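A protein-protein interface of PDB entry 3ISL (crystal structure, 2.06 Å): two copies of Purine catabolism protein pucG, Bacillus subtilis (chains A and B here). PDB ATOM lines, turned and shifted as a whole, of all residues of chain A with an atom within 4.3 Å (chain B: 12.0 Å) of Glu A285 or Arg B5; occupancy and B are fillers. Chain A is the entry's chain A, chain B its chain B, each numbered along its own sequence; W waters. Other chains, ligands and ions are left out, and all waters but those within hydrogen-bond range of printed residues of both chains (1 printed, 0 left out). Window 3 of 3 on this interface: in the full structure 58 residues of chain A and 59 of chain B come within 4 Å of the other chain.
Of the 9 printed residues of chain A, 4 touch a printed residue of chain B.
Printed residues of chain B that touch a printed residue of chain A: Arg B5, Glu B6 and Leu B7.
The side-chain carboxylate (OE2) of Glu A48 lies within salt-bridge range of the guanidinium group (NH2) of Arg B5 (2.4 Å).
NH1 of Arg A277 is in hydrogen-bond range of O of Arg B5 (2.6 Å).
Arg A277 touches Glu B6.
Arg A277 touches Leu B7.
CD of Arg A281 touches O of Arg B5, at 3.5 Å.
NH2 of Arg A281 touches CA of Glu B6, at 3.5 Å.
Glu A285 touches Arg B5.
NH2 of Arg A277 lies within salt-bridge range of OE1 of Glu A48 (2.9 Å).
The guanidinium group (NH1) of Arg A281 lies within salt-bridge range of the side-chain carboxylate (OE2) of Glu A285.
No position is printed for both chains.
Glu A285 touches just one residue of chain B: Arg B5 (3.8 Å).
Of chain A, only Glu A48 (2.4 Å), Arg A277 (2.6 Å), Arg A281 (3.5 Å) and Glu A285 (3.8 Å) come within 4 Å of Arg B5.
Arg A281 touches just these residues of chain B: Arg B5 and Glu B6.
No residue of chain B comes within 4 Å of Leu A282.
No residue of chain B comes within 4 Å of Val A283.
No residue of chain B comes within 4 Å of Leu A284.
No residue of chain B comes within 4 Å of Glu A286.
No residue of chain B comes within 4 Å of Gly A287.
Of the printed residues of chain A, Leu B7 touches Arg A277 (3.6 Å).
Of the printed residues of chain B, Glu A48 touches Arg B5.
Of the printed residues of chain A, Glu B6 touches Arg A277 and Arg A281.
Cys B8 touches none of the printed residues of chain A.
The nearest residue of chain B that does not touch Glu A285 is Glu B6 (5.6 Å).
The nearest printed residue of chain A that does not touch Arg B5 is Leu A284 (7.7 Å).
Water W1 lies within hydrogen-bond range of the backbone carbonyl oxygen of Glu B6 (2.8 Å), the backbone carbonyl oxygen of Arg B5 (3.5 Å) and the guanidinium group of Arg A277 (3.5 Å).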
ATOM      1  N   GLU A  48     -30.253  19.721  16.761  1.00  0.00           N
ATOM      2  CA  GLU A  48     -29.575  18.441  16.896  1.00  0.00           C
ATOM      3  C   GLU A  48     -30.424  17.445  17.675  1.00  0.00           C
ATOM      4  O   GLU A  48     -30.374  16.216  17.453  1.00  0.00           O
ATOM      5  CB  GLU A  48     -28.297  18.679  17.685  1.00  0.00           C
ATOM      6  CG  GLU A  48     -27.363  17.497  17.675  1.00  0.00           C
ATOM      7  CD  GLU A  48     -25.970  17.943  18.067  1.00  0.00           C
ATOM      8  OE1 GLU A  48     -25.874  19.045  18.712  1.00  0.00           O
ATOM      9  OE2 GLU A  48     -25.011  17.200  17.682  1.00  0.00           O
ATOM     10  N   ARG A 277     -31.268  16.043  25.258  1.00  0.00           N
ATOM     11  CA  ARG A 277     -30.121  16.027  24.350  1.00  0.00           C
ATOM     12  C   ARG A 277     -29.032  15.052  24.811  1.00  0.00           C
ATOM     13  O   ARG A 277     -28.643  14.117  24.070  1.00  0.00           O
ATOM     14  CB  ARG A 277     -29.603  17.465  24.224  1.00  0.00           C
ATOM     15  CG  ARG A 277     -28.663  17.795  22.977  1.00  0.00           C
ATOM     16  CD  ARG A 277     -27.228  17.487  23.292  1.00  0.00           C
ATOM     17  NE  ARG A 277     -26.357  17.941  22.206  1.00  0.00           N
ATOM     18  CZ  ARG A 277     -25.062  17.673  22.096  1.00  0.00           C
ATOM     19  NH1 ARG A 277     -24.445  16.986  23.064  1.00  0.00           N
ATOM     20  NH2 ARG A 277     -24.375  18.135  21.029  1.00  0.00           N
ATOM     21  N   ARG A 281     -28.225  11.407  23.276  1.00  0.00           N
ATOM     22  CA  ARG A 281     -26.874  11.170  22.706  1.00  0.00           C
ATOM     23  C   ARG A 281     -26.278   9.858  23.271  1.00  0.00           C
ATOM     24  O   ARG A 281     -25.585   9.169  22.559  1.00  0.00           O
ATOM     25  CB  ARG A 281     -25.931  12.352  22.982  1.00  0.00           C
ATOM     26  CG  ARG A 281     -24.458  12.083  22.762  1.00  0.00           C
ATOM     27  CD  ARG A 281     -23.634  13.296  23.046  1.00  0.00           C
ATOM     28  NE  ARG A 281     -23.546  13.656  24.464  1.00  0.00           N
ATOM     29  CZ  ARG A 281     -22.670  13.154  25.335  1.00  0.00           C
ATOM     30  NH1 ARG A 281     -21.829  12.163  25.012  1.00  0.00           N
ATOM     31  NH2 ARG A 281     -22.680  13.630  26.566  1.00  0.00           N
ATOM     32  N   LEU A 282     -26.503   9.563  24.557  1.00  0.00           N
ATOM     33  CA  LEU A 282     -25.958   8.363  25.180  1.00  0.00           C
ATOM     34  C   LEU A 282     -26.567   7.119  24.634  1.00  0.00           C
ATOM     35  O   LEU A 282     -25.850   6.089  24.470  1.00  0.00           O
ATOM     36  CB  LEU A 282     -26.066   8.343  26.707  1.00  0.00           C
ATOM     37  CG  LEU A 282     -25.329   9.473  27.422  1.00  0.00           C
ATOM     38  CD1 LEU A 282     -25.337   9.268  28.950  1.00  0.00           C
ATOM     39  CD2 LEU A 282     -23.911   9.709  26.937  1.00  0.00           C
ATOM     40  N   VAL A 283     -27.861   7.167  24.340  1.00  0.00           N
ATOM     41  CA  VAL A 283     -28.422   5.982  23.689  1.00  0.00           C
ATOM     42  C   VAL A 283     -27.800   5.689  22.337  1.00  0.00           C
ATOM     43  O   VAL A 283     -27.483   4.568  22.025  1.00  0.00           O
ATOM     44  CB  VAL A 283     -29.982   5.818  23.754  1.00  0.00           C
ATOM     45  CG1 VAL A 283     -30.673   6.738  24.679  1.00  0.00           C
ATOM     46  CG2 VAL A 283     -30.712   5.266  22.431  1.00  0.00           C
ATOM     47  N   LEU A 284     -27.608   6.721  21.569  1.00  0.00           N
ATOM     48  CA  LEU A 284     -27.044   6.573  20.240  1.00  0.00           C
ATOM     49  C   LEU A 284     -25.568   6.192  20.289  1.00  0.00           C
ATOM     50  O   LEU A 284     -25.092   5.602  19.361  1.00  0.00           O
ATOM     51  CB  LEU A 284     -27.264   7.889  19.472  1.00  0.00           C
ATOM     52  CG  LEU A 284     -28.498   8.012  18.558  1.00  0.00           C
ATOM     53  CD1 LEU A 284     -29.641   6.880  18.506  1.00  0.00           C
ATOM     54  CD2 LEU A 284     -29.066   9.361  18.548  1.00  0.00           C
ATOM     55  N   GLU A 285     -24.831   6.557  21.351  1.00  0.00           N
ATOM     56  CA  GLU A 285     -23.448   6.175  21.439  1.00  0.00           C
ATOM     57  C   GLU A 285     -23.350   4.706  21.763  1.00  0.00           C
ATOM     58  O   GLU A 285     -22.455   4.033  21.261  1.00  0.00           O
ATOM     59  CB  GLU A 285     -22.650   6.987  22.445  1.00  0.00           C
ATOM     60  CG  GLU A 285     -22.634   8.497  22.122  1.00  0.00           C
ATOM     61  CD  GLU A 285     -21.679   9.329  23.008  1.00  0.00           C
ATOM     62  OE1 GLU A 285     -21.254   8.811  24.064  1.00  0.00           O
ATOM     63  OE2 GLU A 285     -21.341  10.502  22.608  1.00  0.00           O
ATOM     64  N   GLU A 286     -24.274   4.221  22.607  1.00  0.00           N
ATOM     65  CA  GLU A 286     -24.387   2.821  22.868  1.00  0.00           C
ATOM     66  C   GLU A 286     -24.713   2.035  21.588  1.00  0.00           C
ATOM     67  O   GLU A 286     -24.099   0.980  21.289  1.00  0.00           O
ATOM     68  CB  GLU A 286     -25.414   2.539  23.984  1.00  0.00           C
ATOM     69  CG  GLU A 286     -25.383   1.005  24.387  1.00  0.00           C
ATOM     70  CD  GLU A 286     -26.230   0.652  25.604  1.00  0.00           C
ATOM     71  OE1 GLU A 286     -26.962   1.540  26.099  1.00  0.00           O
ATOM     72  OE2 GLU A 286     -26.167  -0.520  26.124  1.00  0.00           O
ATOM     73  N   GLY A 287     -25.642   2.554  20.789  1.00  0.00           N
ATOM     74  CA  GLY A 287     -26.103   1.779  19.666  1.00  0.00           C
ATOM     75  C   GLY A 287     -27.453   1.208  20.055  1.00  0.00           C
ATOM     76  O   GLY A 287     -27.585   0.501  21.101  1.00  0.00           O
ATOM     77  N   ARG B   5     -18.378  15.990  21.584  1.00  0.00           N
ATOM     78  CA  ARG B   5     -19.857  16.076  21.386  1.00  0.00           C
ATOM     79  C   ARG B   5     -20.775  16.073  22.639  1.00  0.00           C
ATOM     80  O   ARG B   5     -21.968  16.307  22.482  1.00  0.00           O
ATOM     81  CB  ARG B   5     -20.338  15.134  20.294  1.00  0.00           C
ATOM     82  CG  ARG B   5     -20.225  13.666  20.577  1.00  0.00           C
ATOM     83  CD  ARG B   5     -21.205  12.954  19.709  1.00  0.00           C
ATOM     84  NE  ARG B   5     -22.341  13.849  19.467  1.00  0.00           N
ATOM     85  CZ  ARG B   5     -22.436  14.638  18.409  1.00  0.00           C
ATOM     86  NH1 ARG B   5     -21.471  14.627  17.486  1.00  0.00           N
ATOM     87  NH2 ARG B   5     -23.489  15.428  18.273  1.00  0.00           N
ATOM     88  N   GLU B   6     -20.234  15.890  23.849  1.00  0.00           N
ATOM     89  CA  GLU B   6     -20.940  16.329  25.091  1.00  0.00           C
ATOM     90  C   GLU B   6     -21.365  17.839  24.946  1.00  0.00           C
ATOM     91  O   GLU B   6     -20.786  18.579  24.169  1.00  0.00           O
ATOM     92  CB  GLU B   6     -20.016  16.263  26.311  1.00  0.00           C
ATOM     93  CG  GLU B   6     -19.088  17.509  26.287  1.00  0.00           C
ATOM     94  CD  GLU B   6     -17.833  17.396  27.082  1.00  0.00           C
ATOM     95  OE1 GLU B   6     -17.909  17.423  28.337  1.00  0.00           O
ATOM     96  OE2 GLU B   6     -16.770  17.346  26.439  1.00  0.00           O
ATOM     97  N   LEU B   7     -22.388  18.261  25.666  1.00  0.00           N
ATOM     98  CA  LEU B   7     -22.957  19.571  25.457  1.00  0.00           C
ATOM     99  C   LEU B   7     -21.914  20.659  25.759  1.00  0.00           C
ATOM    100  O   LEU B   7     -21.075  20.527  26.658  1.00  0.00           O
ATOM    101  CB  LEU B   7     -24.186  19.737  26.349  1.00  0.00           C
ATOM    102  CG  LEU B   7     -25.044  20.984  26.275  1.00  0.00           C
ATOM    103  CD1 LEU B   7     -26.064  20.856  25.239  1.00  0.00           C
ATOM    104  CD2 LEU B   7     -25.713  21.140  27.630  1.00  0.00           C
ATOM    105  N   CYS B   8     -21.961  21.731  24.993  1.00  0.00           N
ATOM    106  CA  CYS B   8     -21.039  22.831  25.185  1.00  0.00           C
ATOM    107  C   CYS B   8     -21.883  24.027  24.867  1.00  0.00           C
ATOM    108  O   CYS B   8     -22.372  24.154  23.750  1.00  0.00           O
ATOM    109  CB  CYS B   8     -19.858  22.769  24.206  1.00  0.00           C
ATOM    110  SG  CYS B   8     -18.620  24.131  24.540  1.00  0.00           S
ATOM    111  N   THR B   9     -22.061  24.896  25.862  1.00  0.00           N
ATOM    112  CA  THR B   9     -22.803  26.121  25.721  1.00  0.00           C
ATOM    113  C   THR B   9     -22.014  27.325  26.257  1.00  0.00           C
ATOM    114  O   THR B   9     -21.204  27.190  27.147  1.00  0.00           O
ATOM    115  CB  THR B   9     -24.152  26.067  26.534  1.00  0.00           C
ATOM    116  OG1 THR B   9     -23.854  25.573  27.815  1.00  0.00           O
ATOM    117  CG2 THR B   9     -25.154  25.102  25.903  1.00  0.00           C
HETATM  118  O   HOH W   1     -21.249  19.576  21.617  1.00  0.00           O
